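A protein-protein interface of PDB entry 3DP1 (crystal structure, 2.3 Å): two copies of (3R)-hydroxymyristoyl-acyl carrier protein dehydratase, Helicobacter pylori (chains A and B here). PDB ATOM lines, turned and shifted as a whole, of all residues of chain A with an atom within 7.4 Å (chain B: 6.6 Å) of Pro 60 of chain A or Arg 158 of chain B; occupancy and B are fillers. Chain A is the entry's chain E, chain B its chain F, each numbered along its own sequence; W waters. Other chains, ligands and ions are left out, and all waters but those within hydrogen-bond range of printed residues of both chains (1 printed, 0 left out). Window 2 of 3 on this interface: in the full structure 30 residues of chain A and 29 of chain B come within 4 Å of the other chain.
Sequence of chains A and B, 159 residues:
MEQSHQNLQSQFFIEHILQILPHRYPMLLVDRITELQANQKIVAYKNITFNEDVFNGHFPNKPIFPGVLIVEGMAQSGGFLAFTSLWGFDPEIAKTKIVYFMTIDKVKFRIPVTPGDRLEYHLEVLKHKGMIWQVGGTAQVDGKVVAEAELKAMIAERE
Water W1 lies within hydrogen-bond range of NE2 of His 58 of chain A (2.8 Å) and NE2 of His 23 of chain B (3.5 Å).
O of Pro 60 of chain A lies within hydrogen-bond range of NH1 of Arg 158 of chain B, at 3.3 Å.
O of Gly 57 of chain A sits at hydrogen-bond distance from N of Arg 24 of chain B (3.0 Å).
O of Thr 96 of chain B lies within hydrogen-bond range of N of Arg 158 of chain B.
NH2 of Arg 158 of chain B sits at hydrogen-bond distance from O of Lys 97 of chain B.
The backbone NH (N) of Ile 98 of chain B is in hydrogen-bond range of the backbone carbonyl oxygen (O) of Ala 156 of chain B (2.7 Å).
O of Pro 22 of chain B is in hydrogen-bond range of NH2 of Arg 24 of chain B (3.5 Å).
Phe 55 of chain A touches none of the printed residues of chain B.
Of chain B, only Pro 22, Arg 24 and Arg 158 come within 4 Å of Pro 60 of chain A.
Of the printed residues of chain A, Pro 22 of chain B touches Phe 59 and Pro 60.
Printed residues of chain A within 4 Å of His 23 of chain B: Gly 57 (3.6 Å) and Phe 59 (3.5 Å).
Of the printed residues of chain A, Arg 24 of chain B touches Gly 57 and Pro 60.
Printed residues of chain A within 4 Å of Ile 98 of chain B: Phe 59.
Glu 157 of chain B touches none of the printed residues of chain A.
Of chain A, only Pro 60 comes within 4 Å of Arg 158 of chain B.
The nearest residue of chain A that does not touch Arg 158 of chain B is Phe 59 of chain A (4.1 Å).
No position is printed for both chains.
Among the printed residues, pairs that only touch across the chains: Phe 59 of chain A with His 23 of chain B, Phe 59 of chain A with Pro 22 of chain B, Gly 57 of chain A with His 23 of chain B, Pro 60 of chain A with Pro 22 of chain B, Pro 60 of chain A with Arg 24 of chain B and Phe 59 of chain A with Ile 98 of chain B.
Hydrophobic or aromatic side chains of chain B that line the printed part of chain A: Pro 22, His 23 and Ile 98.
Along chain B the printed residues that touch a printed residue of chain A span positions 22 to 158.
Of the 11 printed residues of chain A, 3 touch a printed residue of chain B.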
ATOM      1  N   VAL A  54      20.900  18.121   0.667  1.00  0.00           N
ATOM      2  CA  VAL A  54      22.119  18.850   1.005  1.00  0.00           C
ATOM      3  C   VAL A  54      22.544  19.790  -0.104  1.00  0.00           C
ATOM      4  O   VAL A  54      23.123  20.835   0.164  1.00  0.00           O
ATOM      5  CB  VAL A  54      23.327  17.923   1.297  1.00  0.00           C
ATOM      6  CG1 VAL A  54      23.180  17.301   2.665  1.00  0.00           C
ATOM      7  CG2 VAL A  54      23.451  16.856   0.210  1.00  0.00           C
ATOM      8  N   PHE A  55      22.252  19.422  -1.347  1.00  0.00           N
ATOM      9  CA  PHE A  55      22.639  20.250  -2.484  1.00  0.00           C
ATOM     10  C   PHE A  55      21.962  21.613  -2.578  1.00  0.00           C
ATOM     11  O   PHE A  55      22.417  22.482  -3.321  1.00  0.00           O
ATOM     12  CB  PHE A  55      22.468  19.462  -3.782  1.00  0.00           C
ATOM     13  CG  PHE A  55      23.498  18.384  -3.955  1.00  0.00           C
ATOM     14  CD1 PHE A  55      23.120  17.064  -4.150  1.00  0.00           C
ATOM     15  CD2 PHE A  55      24.854  18.694  -3.893  1.00  0.00           C
ATOM     16  CE1 PHE A  55      24.084  16.061  -4.279  1.00  0.00           C
ATOM     17  CE2 PHE A  55      25.820  17.705  -4.020  1.00  0.00           C
ATOM     18  CZ  PHE A  55      25.433  16.381  -4.214  1.00  0.00           C
ATOM     19  N   ASN A  56      20.880  21.804  -1.830  1.00  0.00           N
ATOM     20  CA  ASN A  56      20.216  23.098  -1.820  1.00  0.00           C
ATOM     21  C   ASN A  56      21.142  24.108  -1.146  1.00  0.00           C
ATOM     22  O   ASN A  56      21.101  25.293  -1.445  1.00  0.00           O
ATOM     23  CB  ASN A  56      18.894  23.029  -1.056  1.00  0.00           C
ATOM     24  CG  ASN A  56      17.775  22.433  -1.884  1.00  0.00           C
ATOM     25  OD1 ASN A  56      17.431  22.957  -2.945  1.00  0.00           O
ATOM     26  ND2 ASN A  56      17.200  21.332  -1.406  1.00  0.00           N
ATOM     27  N   GLY A  57      21.995  23.636  -0.246  1.00  0.00           N
ATOM     28  CA  GLY A  57      22.887  24.557   0.436  1.00  0.00           C
ATOM     29  C   GLY A  57      24.377  24.367   0.222  1.00  0.00           C
ATOM     30  O   GLY A  57      25.172  25.111   0.778  1.00  0.00           O
ATOM     31  N   HIS A  58      24.774  23.410  -0.601  1.00  0.00           N
ATOM     32  CA  HIS A  58      26.198  23.165  -0.789  1.00  0.00           C
ATOM     33  C   HIS A  58      26.579  22.745  -2.212  1.00  0.00           C
ATOM     34  O   HIS A  58      26.827  21.567  -2.452  1.00  0.00           O
ATOM     35  CB  HIS A  58      26.625  22.084   0.211  1.00  0.00           C
ATOM     36  CG  HIS A  58      28.101  21.997   0.437  1.00  0.00           C
ATOM     37  ND1 HIS A  58      28.955  21.358  -0.434  1.00  0.00           N
ATOM     38  CD2 HIS A  58      28.872  22.448   1.456  1.00  0.00           C
ATOM     39  CE1 HIS A  58      30.188  21.416   0.037  1.00  0.00           C
ATOM     40  NE2 HIS A  58      30.165  22.072   1.183  1.00  0.00           N
ATOM     41  N   PHE A  59      26.633  23.687  -3.159  1.00  0.00           N
ATOM     42  CA  PHE A  59      26.347  25.111  -2.950  1.00  0.00           C
ATOM     43  C   PHE A  59      25.336  25.516  -4.015  1.00  0.00           C
ATOM     44  O   PHE A  59      25.237  24.870  -5.052  1.00  0.00           O
ATOM     45  CB  PHE A  59      27.611  25.960  -3.151  1.00  0.00           C
ATOM     46  CG  PHE A  59      28.679  25.736  -2.120  1.00  0.00           C
ATOM     47  CD1 PHE A  59      28.584  26.317  -0.862  1.00  0.00           C
ATOM     48  CD2 PHE A  59      29.782  24.933  -2.406  1.00  0.00           C
ATOM     49  CE1 PHE A  59      29.577  26.100   0.105  1.00  0.00           C
ATOM     50  CE2 PHE A  59      30.777  24.708  -1.452  1.00  0.00           C
ATOM     51  CZ  PHE A  59      30.678  25.289  -0.198  1.00  0.00           C
ATOM     52  N   PRO A  60      24.570  26.589  -3.777  1.00  0.00           N
ATOM     53  CA  PRO A  60      23.599  26.998  -4.796  1.00  0.00           C
ATOM     54  C   PRO A  60      24.286  27.136  -6.165  1.00  0.00           C
ATOM     55  O   PRO A  60      25.317  27.795  -6.282  1.00  0.00           O
ATOM     56  CB  PRO A  60      23.090  28.328  -4.257  1.00  0.00           C
ATOM     57  CG  PRO A  60      23.119  28.100  -2.768  1.00  0.00           C
ATOM     58  CD  PRO A  60      24.470  27.438  -2.578  1.00  0.00           C
ATOM     59  N   ASN A  61      23.717  26.496  -7.182  1.00  0.00           N
ATOM     60  CA  ASN A  61      24.261  26.511  -8.544  1.00  0.00           C
ATOM     61  C   ASN A  61      25.595  25.793  -8.728  1.00  0.00           C
ATOM     62  O   ASN A  61      26.152  25.777  -9.832  1.00  0.00           O
ATOM     63  CB  ASN A  61      24.401  27.946  -9.059  1.00  0.00           C
ATOM     64  CG  ASN A  61      23.064  28.607  -9.284  1.00  0.00           C
ATOM     65  OD1 ASN A  61      22.093  27.956  -9.683  1.00  0.00           O
ATOM     66  ND2 ASN A  61      23.003  29.908  -9.041  1.00  0.00           N
ATOM     67  N   LYS A  62      26.111  25.201  -7.657  1.00  0.00           N
ATOM     68  CA  LYS A  62      27.376  24.489  -7.734  1.00  0.00           C
ATOM     69  C   LYS A  62      27.357  23.309  -6.753  1.00  0.00           C
ATOM     70  O   LYS A  62      27.946  23.372  -5.672  1.00  0.00           O
ATOM     71  CB  LYS A  62      28.514  25.453  -7.403  1.00  0.00           C
ATOM     72  CG  LYS A  62      29.918  24.884  -7.560  1.00  0.00           C
ATOM     73  CD  LYS A  62      30.331  24.762  -9.018  1.00  0.00           C
ATOM     74  CE  LYS A  62      31.822  24.459  -9.121  1.00  0.00           C
ATOM     75  NZ  LYS A  62      32.262  24.207 -10.522  1.00  0.00           N
ATOM     76  N   PRO A  63      26.666  22.215  -7.127  1.00  0.00           N
ATOM     77  CA  PRO A  63      26.540  21.000  -6.316  1.00  0.00           C
ATOM     78  C   PRO A  63      27.854  20.280  -6.009  1.00  0.00           C
ATOM     79  O   PRO A  63      28.485  19.709  -6.896  1.00  0.00           O
ATOM     80  CB  PRO A  63      25.600  20.120  -7.147  1.00  0.00           C
ATOM     81  CG  PRO A  63      24.795  21.109  -7.930  1.00  0.00           C
ATOM     82  CD  PRO A  63      25.831  22.119  -8.338  1.00  0.00           C
ATOM     83  N   ILE A  64      28.246  20.310  -4.739  1.00  0.00           N
ATOM     84  CA  ILE A  64      29.454  19.646  -4.270  1.00  0.00           C
ATOM     85  C   ILE A  64      29.084  18.815  -3.040  1.00  0.00           C
ATOM     86  O   ILE A  64      28.647  19.366  -2.027  1.00  0.00           O
ATOM     87  CB  ILE A  64      30.523  20.663  -3.850  1.00  0.00           C
ATOM     88  CG1 ILE A  64      30.926  21.529  -5.050  1.00  0.00           C
ATOM     89  CG2 ILE A  64      31.727  19.929  -3.278  1.00  0.00           C
ATOM     90  CD1 ILE A  64      31.773  22.736  -4.675  1.00  0.00           C
ATOM     91  N   PRO B  22      29.045  31.179   1.360  1.00  0.00           N
ATOM     92  CA  PRO B  22      28.193  30.707   0.267  1.00  0.00           C
ATOM     93  C   PRO B  22      27.205  29.648   0.740  1.00  0.00           C
ATOM     94  O   PRO B  22      26.169  29.441   0.111  1.00  0.00           O
ATOM     95  CB  PRO B  22      29.195  30.140  -0.724  1.00  0.00           C
ATOM     96  CG  PRO B  22      30.236  29.539   0.198  1.00  0.00           C
ATOM     97  CD  PRO B  22      30.405  30.622   1.250  1.00  0.00           C
ATOM     98  N   HIS B  23      27.528  28.985   1.850  1.00  0.00           N
ATOM     99  CA  HIS B  23      26.665  27.934   2.388  1.00  0.00           C
ATOM    100  C   HIS B  23      25.229  28.393   2.636  1.00  0.00           C
ATOM    101  O   HIS B  23      24.976  29.530   3.038  1.00  0.00           O
ATOM    102  CB  HIS B  23      27.226  27.384   3.700  1.00  0.00           C
ATOM    103  CG  HIS B  23      28.683  27.055   3.646  1.00  0.00           C
ATOM    104  ND1 HIS B  23      29.664  28.025   3.651  1.00  0.00           N
ATOM    105  CD2 HIS B  23      29.327  25.867   3.588  1.00  0.00           C
ATOM    106  CE1 HIS B  23      30.850  27.446   3.598  1.00  0.00           C
ATOM    107  NE2 HIS B  23      30.673  26.139   3.558  1.00  0.00           N
ATOM    108  N   ARG B  24      24.294  27.486   2.396  1.00  0.00           N
ATOM    109  CA  ARG B  24      22.884  27.764   2.612  1.00  0.00           C
ATOM    110  C   ARG B  24      22.229  26.532   3.206  1.00  0.00           C
ATOM    111  O   ARG B  24      22.888  25.516   3.417  1.00  0.00           O
ATOM    112  CB  ARG B  24      22.202  28.150   1.301  1.00  0.00           C
ATOM    113  CG  ARG B  24      22.639  29.510   0.772  1.00  0.00           C
ATOM    114  CD  ARG B  24      22.165  30.624   1.685  1.00  0.00           C
ATOM    115  NE  ARG B  24      22.457  31.948   1.142  1.00  0.00           N
ATOM    116  CZ  ARG B  24      23.625  32.571   1.262  1.00  0.00           C
ATOM    117  NH1 ARG B  24      23.789  33.775   0.727  1.00  0.00           N
ATOM    118  NH2 ARG B  24      24.624  32.000   1.922  1.00  0.00           N
ATOM    119  N   ALA B  94      32.757  38.174  -1.906  1.00  0.00           N
ATOM    120  CA  ALA B  94      32.262  36.908  -1.387  1.00  0.00           C
ATOM    121  C   ALA B  94      31.350  36.151  -2.355  1.00  0.00           C
ATOM    122  O   ALA B  94      31.537  34.947  -2.575  1.00  0.00           O
ATOM    123  CB  ALA B  94      31.532  37.142  -0.079  1.00  0.00           C
ATOM    124  N   LYS B  95      30.374  36.848  -2.943  1.00  0.00           N
ATOM    125  CA  LYS B  95      29.416  36.202  -3.840  1.00  0.00           C
ATOM    126  C   LYS B  95      30.000  35.422  -5.009  1.00  0.00           C
ATOM    127  O   LYS B  95      29.273  34.670  -5.674  1.00  0.00           O
ATOM    128  CB  LYS B  95      28.395  37.215  -4.379  1.00  0.00           C
ATOM    129  CG  LYS B  95      28.976  38.249  -5.329  1.00  0.00           C
ATOM    130  CD  LYS B  95      27.885  39.140  -5.918  1.00  0.00           C
ATOM    131  CE  LYS B  95      28.506  40.296  -6.712  1.00  0.00           C
ATOM    132  NZ  LYS B  95      29.556  39.832  -7.686  1.00  0.00           N
ATOM    133  N   THR B  96      31.293  35.578  -5.275  1.00  0.00           N
ATOM    134  CA  THR B  96      31.900  34.840  -6.383  1.00  0.00           C
ATOM    135  C   THR B  96      32.710  33.646  -5.899  1.00  0.00           C
ATOM    136  O   THR B  96      33.190  32.835  -6.707  1.00  0.00           O
ATOM    137  CB  THR B  96      32.847  35.718  -7.199  1.00  0.00           C
ATOM    138  OG1 THR B  96      33.863  36.242  -6.333  1.00  0.00           O
ATOM    139  CG2 THR B  96      32.088  36.848  -7.858  1.00  0.00           C
ATOM    140  N   LYS B  97      32.854  33.532  -4.581  1.00  0.00           N
ATOM    141  CA  LYS B  97      33.638  32.453  -4.000  1.00  0.00           C
ATOM    142  C   LYS B  97      32.847  31.327  -3.366  1.00  0.00           C
ATOM    143  O   LYS B  97      31.657  31.457  -3.081  1.00  0.00           O
ATOM    144  CB  LYS B  97      34.599  33.016  -2.949  1.00  0.00           C
ATOM    145  CG  LYS B  97      35.854  33.686  -3.495  1.00  0.00           C
ATOM    146  CD  LYS B  97      35.537  34.851  -4.385  1.00  0.00           C
ATOM    147  CE  LYS B  97      36.756  35.753  -4.597  1.00  0.00           C
ATOM    148  NZ  LYS B  97      37.886  35.060  -5.280  1.00  0.00           N
ATOM    149  N   ILE B  98      33.540  30.206  -3.179  1.00  0.00           N
ATOM    150  CA  ILE B  98      33.020  29.018  -2.507  1.00  0.00           C
ATOM    151  C   ILE B  98      34.207  28.547  -1.690  1.00  0.00           C
ATOM    152  O   ILE B  98      35.287  29.141  -1.753  1.00  0.00           O
ATOM    153  CB  ILE B  98      32.573  27.877  -3.470  1.00  0.00           C
ATOM    154  CG1 ILE B  98      33.654  27.592  -4.516  1.00  0.00           C
ATOM    155  CG2 ILE B  98      31.228  28.229  -4.099  1.00  0.00           C
ATOM    156  CD1 ILE B  98      33.321  26.412  -5.432  1.00  0.00           C
ATOM    157  N   ALA B 156      37.815  29.650  -3.155  1.00  0.00           N
ATOM    158  CA  ALA B 156      37.935  29.639  -4.607  1.00  0.00           C
ATOM    159  C   ALA B 156      36.799  30.361  -5.329  1.00  0.00           C
ATOM    160  O   ALA B 156      35.746  30.645  -4.738  1.00  0.00           O
ATOM    161  CB  ALA B 156      38.020  28.196  -5.098  1.00  0.00           C
ATOM    162  N   GLU B 157      37.038  30.654  -6.608  1.00  0.00           N
ATOM    163  CA  GLU B 157      36.069  31.314  -7.477  1.00  0.00           C
ATOM    164  C   GLU B 157      35.062  30.261  -7.925  1.00  0.00           C
ATOM    165  O   GLU B 157      35.462  29.172  -8.348  1.00  0.00           O
ATOM    166  CB  GLU B 157      36.778  31.886  -8.706  1.00  0.00           C
ATOM    167  CG  GLU B 157      37.494  33.208  -8.473  1.00  0.00           C
ATOM    168  CD  GLU B 157      36.528  34.382  -8.356  1.00  0.00           C
ATOM    169  OE1 GLU B 157      35.693  34.567  -9.280  1.00  0.00           O
ATOM    170  OE2 GLU B 157      36.599  35.122  -7.340  1.00  0.00           O
ATOM    171  N   ARG B 158      33.766  30.573  -7.837  1.00  0.00           N
ATOM    172  CA  ARG B 158      32.731  29.617  -8.243  1.00  0.00           C
ATOM    173  C   ARG B 158      33.016  29.119  -9.662  1.00  0.00           C
ATOM    174  O   ARG B 158      33.530  29.945 -10.458  1.00  0.00           O
ATOM    175  CB  ARG B 158      31.342  30.264  -8.227  1.00  0.00           C
ATOM    176  CG  ARG B 158      31.010  31.110  -7.009  1.00  0.00           C
ATOM    177  CD  ARG B 158      29.576  31.664  -7.128  1.00  0.00           C
ATOM    178  NE  ARG B 158      28.595  30.745  -6.549  1.00  0.00           N
ATOM    179  CZ  ARG B 158      28.379  30.621  -5.239  1.00  0.00           C
ATOM    180  NH1 ARG B 158      27.469  29.752  -4.794  1.00  0.00           N
ATOM    181  NH2 ARG B 158      29.062  31.384  -4.376  1.00  0.00           N
HETATM  182  O   HOH W   1      31.724  22.809   3.366  1.00  0.00           O
